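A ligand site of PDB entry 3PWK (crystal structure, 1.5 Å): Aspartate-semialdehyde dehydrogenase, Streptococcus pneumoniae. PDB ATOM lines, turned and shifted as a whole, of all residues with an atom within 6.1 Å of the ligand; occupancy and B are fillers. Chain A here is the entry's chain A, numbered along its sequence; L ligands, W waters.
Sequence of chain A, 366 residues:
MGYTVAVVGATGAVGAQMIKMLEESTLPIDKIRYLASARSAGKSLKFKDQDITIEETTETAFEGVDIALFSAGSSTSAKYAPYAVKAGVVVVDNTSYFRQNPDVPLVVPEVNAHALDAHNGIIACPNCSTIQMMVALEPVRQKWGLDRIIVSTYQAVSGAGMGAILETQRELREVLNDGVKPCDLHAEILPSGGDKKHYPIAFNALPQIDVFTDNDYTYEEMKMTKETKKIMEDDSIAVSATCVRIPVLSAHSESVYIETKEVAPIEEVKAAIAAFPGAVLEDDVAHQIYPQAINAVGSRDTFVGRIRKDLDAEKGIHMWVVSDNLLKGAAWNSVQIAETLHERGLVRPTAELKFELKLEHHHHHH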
ATOM      1  N   VAL A   8     -25.261 -18.246  -5.079  1.00  0.00           N
ATOM      2  CA  VAL A   8     -25.425 -19.082  -6.271  1.00  0.00           C
ATOM      3  C   VAL A   8     -24.082 -19.169  -6.972  1.00  0.00           C
ATOM      4  O   VAL A   8     -23.533 -18.154  -7.417  1.00  0.00           O
ATOM      5  CB  VAL A   8     -26.502 -18.518  -7.235  1.00  0.00           C
ATOM      6  CG1 VAL A   8     -26.735 -19.470  -8.399  1.00  0.00           C
ATOM      7  CG2 VAL A   8     -27.826 -18.270  -6.515  1.00  0.00           C
ATOM      8  N   GLY A   9     -23.545 -20.383  -7.071  1.00  0.00           N
ATOM      9  CA  GLY A   9     -22.165 -20.578  -7.487  1.00  0.00           C
ATOM     10  C   GLY A   9     -21.235 -20.694  -6.283  1.00  0.00           C
ATOM     11  O   GLY A   9     -20.093 -20.249  -6.354  1.00  0.00           O
ATOM     12  N   ALA A  10     -21.707 -21.314  -5.202  1.00  0.00           N
ATOM     13  CA  ALA A  10     -20.950 -21.311  -3.947  1.00  0.00           C
ATOM     14  C   ALA A  10     -19.626 -22.064  -4.019  1.00  0.00           C
ATOM     15  O   ALA A  10     -18.715 -21.790  -3.250  1.00  0.00           O
ATOM     16  CB  ALA A  10     -21.816 -21.854  -2.797  1.00  0.00           C
ATOM     17  N   THR A  11     -19.535 -23.007  -4.960  1.00  0.00           N
ATOM     18  CA  THR A  11     -18.403 -23.907  -5.074  1.00  0.00           C
ATOM     19  C   THR A  11     -17.267 -23.359  -5.949  1.00  0.00           C
ATOM     20  O   THR A  11     -16.173 -23.967  -6.004  1.00  0.00           O
ATOM     21  CB  THR A  11     -18.842 -25.259  -5.656  1.00  0.00           C
ATOM     22  OG1 THR A  11     -19.628 -25.015  -6.828  1.00  0.00           O
ATOM     23  CG2 THR A  11     -19.673 -26.052  -4.643  1.00  0.00           C
ATOM     24  N   GLY A  12     -17.515 -22.237  -6.641  1.00  0.00           N
ATOM     25  CA  GLY A  12     -16.563 -21.694  -7.609  1.00  0.00           C
ATOM     26  C   GLY A  12     -15.527 -20.802  -6.964  1.00  0.00           C
ATOM     27  O   GLY A  12     -15.553 -20.598  -5.748  1.00  0.00           O
ATOM     28  N   ALA A  13     -14.633 -20.251  -7.782  1.00  0.00           N
ATOM     29  CA  ALA A  13     -13.579 -19.377  -7.262  1.00  0.00           C
ATOM     30  C   ALA A  13     -14.158 -18.100  -6.637  1.00  0.00           C
ATOM     31  O   ALA A  13     -13.763 -17.721  -5.527  1.00  0.00           O
ATOM     32  CB  ALA A  13     -12.578 -19.046  -8.354  1.00  0.00           C
ATOM     33  N   VAL A  14     -15.071 -17.430  -7.340  1.00  0.00           N
ATOM     34  CA  VAL A  14     -15.728 -16.257  -6.751  1.00  0.00           C
ATOM     35  C   VAL A  14     -16.615 -16.669  -5.564  1.00  0.00           C
ATOM     36  O   VAL A  14     -16.615 -16.009  -4.520  1.00  0.00           O
ATOM     37  CB  VAL A  14     -16.559 -15.460  -7.794  1.00  0.00           C
ATOM     38  CG1 VAL A  14     -17.396 -14.392  -7.100  1.00  0.00           C
ATOM     39  CG2 VAL A  14     -15.653 -14.843  -8.855  1.00  0.00           C
ATOM     40  N   LEU A  35     -25.995 -22.531  -3.180  1.00  0.00           N
ATOM     41  CA  LEU A  35     -26.582 -23.098  -4.394  1.00  0.00           C
ATOM     42  C   LEU A  35     -25.522 -23.249  -5.459  1.00  0.00           C
ATOM     43  O   LEU A  35     -24.630 -22.405  -5.609  1.00  0.00           O
ATOM     44  CB  LEU A  35     -27.735 -22.215  -4.902  1.00  0.00           C
ATOM     45  CG  LEU A  35     -29.109 -22.349  -4.250  1.00  0.00           C
ATOM     46  CD1 LEU A  35     -29.107 -22.023  -2.755  1.00  0.00           C
ATOM     47  CD2 LEU A  35     -30.099 -21.451  -4.960  1.00  0.00           C
ATOM     48  N   ALA A  36     -25.603 -24.359  -6.212  1.00  0.00           N
ATOM     49  CA  ALA A  36     -24.720 -24.577  -7.348  1.00  0.00           C
ATOM     50  C   ALA A  36     -25.445 -25.476  -8.342  1.00  0.00           C
ATOM     51  O   ALA A  36     -26.668 -25.416  -8.438  1.00  0.00           O
ATOM     52  CB  ALA A  36     -23.370 -25.152  -6.900  1.00  0.00           C
ATOM     53  N   SER A  37     -24.719 -26.307  -9.086  1.00  0.00           N
ATOM     54  CA  SER A  37     -25.347 -27.191 -10.078  1.00  0.00           C
ATOM     55  C   SER A  37     -25.722 -28.518  -9.438  1.00  0.00           C
ATOM     56  O   SER A  37     -25.311 -28.817  -8.314  1.00  0.00           O
ATOM     57  CB  SER A  37     -24.428 -27.420 -11.284  1.00  0.00           C
ATOM     58  OG  SER A  37     -23.406 -28.365 -10.970  1.00  0.00           O
ATOM     59  N   ALA A  38     -26.499 -29.305 -10.182  1.00  0.00           N
ATOM     60  CA  ALA A  38     -26.931 -30.642  -9.739  1.00  0.00           C
ATOM     61  C   ALA A  38     -25.805 -31.538  -9.209  1.00  0.00           C
ATOM     62  O   ALA A  38     -26.019 -32.303  -8.278  1.00  0.00           O
ATOM     63  CB  ALA A  38     -27.676 -31.341 -10.878  1.00  0.00           C
ATOM     64  N   ARG A  39     -24.604 -31.418  -9.789  1.00  0.00           N
ATOM     65  CA  ARG A  39     -23.474 -32.266  -9.390  1.00  0.00           C
ATOM     66  C   ARG A  39     -22.864 -31.869  -8.046  1.00  0.00           C
ATOM     67  O   ARG A  39     -22.087 -32.629  -7.456  1.00  0.00           O
ATOM     68  CB  ARG A  39     -22.386 -32.300 -10.470  1.00  0.00           C
ATOM     69  CG  ARG A  39     -21.603 -31.012 -10.598  1.00  0.00           C
ATOM     70  CD  ARG A  39     -20.593 -31.098 -11.711  1.00  0.00           C
ATOM     71  NE  ARG A  39     -19.928 -29.811 -11.922  1.00  0.00           N
ATOM     72  CZ  ARG A  39     -18.999 -29.592 -12.852  1.00  0.00           C
ATOM     73  NH1 ARG A  39     -18.627 -30.577 -13.664  1.00  0.00           N
ATOM     74  NH2 ARG A  39     -18.447 -28.386 -12.962  1.00  0.00           N
ATOM     75  N   SER A  40     -23.218 -30.687  -7.552  1.00  0.00           N
ATOM     76  CA  SER A  40     -22.777 -30.234  -6.236  1.00  0.00           C
ATOM     77  C   SER A  40     -23.803 -30.465  -5.138  1.00  0.00           C
ATOM     78  O   SER A  40     -23.444 -30.417  -3.948  1.00  0.00           O
ATOM     79  CB  SER A  40     -22.403 -28.750  -6.276  1.00  0.00           C
ATOM     80  OG  SER A  40     -21.173 -28.567  -6.942  1.00  0.00           O
ATOM     81  N   ALA A  41     -25.060 -30.721  -5.509  1.00  0.00           N
ATOM     82  CA  ALA A  41     -26.136 -30.858  -4.509  1.00  0.00           C
ATOM     83  C   ALA A  41     -25.852 -31.985  -3.525  1.00  0.00           C
ATOM     84  O   ALA A  41     -25.438 -33.078  -3.934  1.00  0.00           O
ATOM     85  CB  ALA A  41     -27.479 -31.055  -5.183  1.00  0.00           C
ATOM     86  N   LYS A  43     -23.506 -32.030  -1.203  1.00  0.00           N
ATOM     87  CA  LYS A  43     -22.205 -31.771  -0.593  1.00  0.00           C
ATOM     88  C   LYS A  43     -22.347 -30.708   0.495  1.00  0.00           C
ATOM     89  O   LYS A  43     -23.365 -30.006   0.563  1.00  0.00           O
ATOM     90  CB  LYS A  43     -21.203 -31.294  -1.640  1.00  0.00           C
ATOM     91  CG  LYS A  43     -20.599 -32.406  -2.505  1.00  0.00           C
ATOM     92  CD  LYS A  43     -19.706 -31.807  -3.593  1.00  0.00           C
ATOM     93  CE  LYS A  43     -18.547 -30.981  -3.010  1.00  0.00           C
ATOM     94  NZ  LYS A  43     -17.959 -30.039  -4.003  1.00  0.00           N
ATOM     95  N   THR A  57     -29.514 -25.301  -8.063  1.00  0.00           N
ATOM     96  CA  THR A  57     -30.176 -24.083  -8.495  1.00  0.00           C
ATOM     97  C   THR A  57     -31.308 -24.394  -9.475  1.00  0.00           C
ATOM     98  O   THR A  57     -31.074 -24.994 -10.532  1.00  0.00           O
ATOM     99  CB  THR A  57     -29.164 -23.104  -9.115  1.00  0.00           C
ATOM    100  OG1 THR A  57     -28.045 -22.956  -8.230  1.00  0.00           O
ATOM    101  CG2 THR A  57     -29.785 -21.727  -9.335  1.00  0.00           C
ATOM    102  N   SER A  71     -22.800 -15.849  -8.788  1.00  0.00           N
ATOM    103  CA  SER A  71     -21.557 -15.919  -9.555  1.00  0.00           C
ATOM    104  C   SER A  71     -21.389 -17.331 -10.053  1.00  0.00           C
ATOM    105  O   SER A  71     -20.510 -18.089  -9.604  1.00  0.00           O
ATOM    106  CB  SER A  71     -20.343 -15.498  -8.733  1.00  0.00           C
ATOM    107  OG  SER A  71     -19.278 -15.232  -9.634  1.00  0.00           O
ATOM    108  N   ALA A  72     -22.239 -17.677 -11.007  1.00  0.00           N
ATOM    109  CA  ALA A  72     -22.303 -19.036 -11.507  1.00  0.00           C
ATOM    110  C   ALA A  72     -22.351 -19.040 -13.043  1.00  0.00           C
ATOM    111  O   ALA A  72     -22.810 -20.004 -13.662  1.00  0.00           O
ATOM    112  CB  ALA A  72     -23.531 -19.719 -10.909  1.00  0.00           C
ATOM    113  N   GLY A  73     -21.856 -17.952 -13.652  1.00  0.00           N
ATOM    114  CA  GLY A  73     -21.823 -17.852 -15.117  1.00  0.00           C
ATOM    115  C   GLY A  73     -23.042 -17.148 -15.677  1.00  0.00           C
ATOM    116  O   GLY A  73     -24.127 -17.217 -15.090  1.00  0.00           O
ATOM    117  N   THR A  76     -26.423 -18.963 -16.024  1.00  0.00           N
ATOM    118  CA  THR A  76     -27.137 -19.298 -14.817  1.00  0.00           C
ATOM    119  C   THR A  76     -27.911 -18.074 -14.331  1.00  0.00           C
ATOM    120  O   THR A  76     -29.028 -18.198 -13.820  1.00  0.00           O
ATOM    121  CB  THR A  76     -26.168 -19.800 -13.737  1.00  0.00           C
ATOM    122  OG1 THR A  76     -25.398 -20.879 -14.294  1.00  0.00           O
ATOM    123  CG2 THR A  76     -26.919 -20.269 -12.505  1.00  0.00           C
ATOM    124  N   LYS A  79     -30.938 -17.565 -16.646  1.00  0.00           N
ATOM    125  CA  LYS A  79     -31.978 -18.553 -16.403  1.00  0.00           C
ATOM    126  C   LYS A  79     -32.729 -18.295 -15.104  1.00  0.00           C
ATOM    127  O   LYS A  79     -33.959 -18.314 -15.077  1.00  0.00           O
ATOM    128  CB  LYS A  79     -31.403 -19.972 -16.370  1.00  0.00           C
ATOM    129  CG  LYS A  79     -31.066 -20.554 -17.730  1.00  0.00           C
ATOM    130  CD  LYS A  79     -30.314 -21.863 -17.544  1.00  0.00           C
ATOM    131  CE  LYS A  79     -29.526 -22.254 -18.780  1.00  0.00           C
ATOM    132  NZ  LYS A  79     -28.537 -23.303 -18.433  1.00  0.00           N
ATOM    133  N   TYR A  80     -32.001 -18.007 -14.022  1.00  0.00           N
ATOM    134  CA  TYR A  80     -32.608 -18.016 -12.687  1.00  0.00           C
ATOM    135  C   TYR A  80     -32.810 -16.675 -11.991  1.00  0.00           C
ATOM    136  O   TYR A  80     -33.675 -16.550 -11.140  1.00  0.00           O
ATOM    137  CB  TYR A  80     -31.834 -18.987 -11.770  1.00  0.00           C
ATOM    138  CG  TYR A  80     -31.755 -20.376 -12.351  1.00  0.00           C
ATOM    139  CD1 TYR A  80     -32.887 -21.179 -12.423  1.00  0.00           C
ATOM    140  CD2 TYR A  80     -30.555 -20.886 -12.844  1.00  0.00           C
ATOM    141  CE1 TYR A  80     -32.839 -22.456 -12.959  1.00  0.00           C
ATOM    142  CE2 TYR A  80     -30.481 -22.169 -13.388  1.00  0.00           C
ATOM    143  CZ  TYR A  80     -31.631 -22.947 -13.439  1.00  0.00           C
ATOM    144  OH  TYR A  80     -31.596 -24.219 -13.971  1.00  0.00           O
ATOM    145  N   SER A 158      -7.221 -16.406 -12.025  1.00  0.00           N
ATOM    146  CA  SER A 158      -8.397 -16.820 -11.227  1.00  0.00           C
ATOM    147  C   SER A 158      -9.655 -16.136 -11.746  1.00  0.00           C
ATOM    148  O   SER A 158     -10.756 -16.589 -11.459  1.00  0.00           O
ATOM    149  CB  SER A 158      -8.200 -16.547  -9.747  1.00  0.00           C
ATOM    150  OG  SER A 158      -8.073 -15.157  -9.492  1.00  0.00           O
ATOM    151  N   ALA A 160     -10.715 -16.355 -14.601  1.00  0.00           N
ATOM    152  CA  ALA A 160     -11.311 -17.318 -15.519  1.00  0.00           C
ATOM    153  C   ALA A 160     -11.855 -18.557 -14.809  1.00  0.00           C
ATOM    154  O   ALA A 160     -12.326 -19.488 -15.452  1.00  0.00           O
ATOM    155  CB  ALA A 160     -10.301 -17.704 -16.584  1.00  0.00           C
ATOM    156  N   GLY A 161     -11.813 -18.566 -13.479  1.00  0.00           N
ATOM    157  CA  GLY A 161     -12.414 -19.633 -12.689  1.00  0.00           C
ATOM    158  C   GLY A 161     -11.415 -20.597 -12.089  1.00  0.00           C
ATOM    159  O   GLY A 161     -10.214 -20.545 -12.386  1.00  0.00           O
ATOM    160  N   MET A 162     -11.908 -21.495 -11.247  1.00  0.00           N
ATOM    161  CA  MET A 162     -11.059 -22.439 -10.558  1.00  0.00           C
ATOM    162  C   MET A 162     -10.231 -23.312 -11.504  1.00  0.00           C
ATOM    163  O   MET A 162      -9.067 -23.601 -11.220  1.00  0.00           O
ATOM    164  CB  MET A 162     -11.893 -23.336  -9.631  1.00  0.00           C
ATOM    165  CG  MET A 162     -11.076 -23.827  -8.483  1.00  0.00           C
ATOM    166  SD  MET A 162     -10.898 -22.538  -7.231  1.00  0.00           S
ATOM    167  CE  MET A 162     -12.353 -22.892  -6.221  1.00  0.00           C
ATOM    168  N   GLY A 163     -10.838 -23.737 -12.614  1.00  0.00           N
ATOM    169  CA  GLY A 163     -10.132 -24.618 -13.554  1.00  0.00           C
ATOM    170  C   GLY A 163      -8.894 -23.948 -14.134  1.00  0.00           C
ATOM    171  O   GLY A 163      -7.853 -24.596 -14.323  1.00  0.00           O
HETATM  172  O1  LIG L   1     -15.994 -20.424 -12.665  1.00  0.00           O
HETATM  173  P1  LIG L   1     -15.758 -21.442 -11.564  1.00  0.00           P
HETATM  174  O2  LIG L   1     -14.723 -21.021 -10.549  1.00  0.00           O
HETATM  175  O3  LIG L   1     -15.608 -22.850 -12.071  1.00  0.00           O
HETATM  176  O4  LIG L   1     -17.175 -21.480 -10.790  1.00  0.00           O
HETATM  177  C1  LIG L   1     -18.383 -21.714 -11.491  1.00  0.00           C
HETATM  178  C2  LIG L   1     -19.518 -21.845 -10.488  1.00  0.00           C
HETATM  179  O5  LIG L   1     -20.732 -21.851 -11.240  1.00  0.00           O
HETATM  180  C3  LIG L   1     -21.531 -22.953 -10.809  1.00  0.00           C
HETATM  181  N1  LIG L   1     -22.419 -23.405 -11.890  1.00  0.00           N
HETATM  182  C4  LIG L   1     -22.078 -23.799 -13.129  1.00  0.00           C
HETATM  183  N2  LIG L   1     -23.189 -24.152 -13.807  1.00  0.00           N
HETATM  184  C5  LIG L   1     -24.233 -23.969 -12.966  1.00  0.00           C
HETATM  185  C6  LIG L   1     -23.738 -23.501 -11.761  1.00  0.00           C
HETATM  186  N3  LIG L   1     -24.574 -23.226 -10.724  1.00  0.00           N
HETATM  187  C7  LIG L   1     -25.897 -23.408 -10.880  1.00  0.00           C
HETATM  188  N4  LIG L   1     -26.402 -23.873 -12.045  1.00  0.00           N
HETATM  189  C8  LIG L   1     -25.606 -24.159 -13.100  1.00  0.00           C
HETATM  190  N5  LIG L   1     -26.136 -24.616 -14.257  1.00  0.00           N
HETATM  191  C9  LIG L   1     -20.503 -24.013 -10.451  1.00  0.00           C
HETATM  192  O6  LIG L   1     -21.087 -25.042  -9.636  1.00  0.00           O
HETATM  193  C10 LIG L   1     -19.498 -23.153  -9.704  1.00  0.00           C
HETATM  194  O7  LIG L   1     -19.995 -22.891  -8.376  1.00  0.00           O
HETATM  195  P2  LIG L   1     -20.651 -26.612  -9.697  1.00  0.00           P
HETATM  196  O8  LIG L   1     -19.470 -26.656  -8.762  1.00  0.00           O
HETATM  197  O9  LIG L   1     -20.310 -26.947 -11.139  1.00  0.00           O
HETATM  198  O10 LIG L   1     -21.892 -27.313  -9.171  1.00  0.00           O
HETATM  199  O   HOH W   1     -15.588 -18.128 -10.191  1.00  0.00           O
HETATM  200  O   HOH W   2     -13.620 -23.445 -13.553  1.00  0.00           O
HETATM  201  O   HOH W   3     -21.576 -27.134 -13.526  1.00  0.00           O
HETATM  202  O   HOH W   4     -28.450 -25.612 -11.693  1.00  0.00           O
HETATM  203  O   HOH W   5     -29.138 -24.968 -15.105  1.00  0.00           O
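Ala 10 touches the ligand. Ala 36 touches the ligand. Thr 57 touches the ligand (OG1 to C7, 3.4 Å). Ser 71 touches the ligand (O to C2, 3.98 Å). Ala 72 touches the ligand. OG1 of Thr 76 touches C8 of the ligand (3.5 Å). CA of Gly 161 touches O2 of the ligand, at 3.4 Å. Within 4 Å of the ligand: Gly 9, Ala 10, Thr 11, Gly 12, Ala 13, Ala 36, Ser 37, Arg 39, Ser 40, Thr 57, Ser 71, Ala 72, Thr 76, Gly 161 and Met 162. The nearest printed residue that does not touch the ligand is Tyr 80 (4.6 Å).
N of Gly 12 lies within hydrogen-bond range of O7 of the ligand (3.1 Å). N of Ser 37 sits at hydrogen-bond distance from O10 of the ligand, 3.0 Å away. An oxygen (O7) of the ligand sits close to the backbone carbonyl oxygen of Gly 9 (3.3 Å). The backbone NH (N) of Ala 13 is in hydrogen-bond range of an oxygen (O2) of the ligand (2.9 Å). OG1 of Thr 11 sits at hydrogen-bond distance from O8 of the ligand (2.5 Å). O10 of the ligand lies within hydrogen-bond range of OG of Ser 37, at 2.6 Å. An oxygen (O10) of the ligand is in hydrogen-bond range of the side-chain hydroxyl (OG) of Ser 40 (2.7 Å). An oxygen (O7) of the ligand is in hydrogen-bond range of the backbone NH of Thr 11 (3.4 Å). The backbone NH of Met 162 is in hydrogen-bond range of an oxygen (O2) of the ligand (2.9 Å). The guanidinium group of Arg 39 is in salt-bridge range of an oxygen (O9) of the ligand (3.0 Å).
The side-chain hydroxyl of Thr 76 is in hydrogen-bond range of the backbone carbonyl oxygen of Ala 72. The backbone carbonyl oxygen of Leu 35 is in hydrogen-bond range of the backbone NH of Gly 9 (2.7 Å). The backbone NH (N) of Arg 39 sits close to the side-chain hydroxyl (OG) of Ser 37, at 3.5 Å. N of Ala 10 is in hydrogen-bond range of O of Leu 35 (3.1 Å). O of Val 8 sits at hydrogen-bond distance from N of Ser 71 (2.8 Å). The backbone carbonyl oxygen of Ala 36 is in hydrogen-bond range of the side-chain hydroxyl of Thr 57, 2.8 Å away.
Water W2 lies within hydrogen-bond range of an oxygen (O3) of the ligand (2.5 Å), the backbone NH of Gly 163 (3.0 Å) and the backbone NH of Met 162 (3.5 Å). Water W3 lies within hydrogen-bond range of O9 of the ligand, OG of Ser 37 and NH2 of Arg 39. Water W4 lies within hydrogen-bond range of a nitrogen (N4) of the ligand (2.7 Å) and the backbone carbonyl oxygen of Thr 57 (2.9 Å). Water W1 lies within hydrogen-bond range of N of Val 14 (3.0 Å), O2 of the ligand (3.0 Å) and N of Ala 13 (3.3 Å). Water W5 lies within hydrogen-bond range of OH of Tyr 80 (2.8 Å) and N5 of the ligand (3.1 Å).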
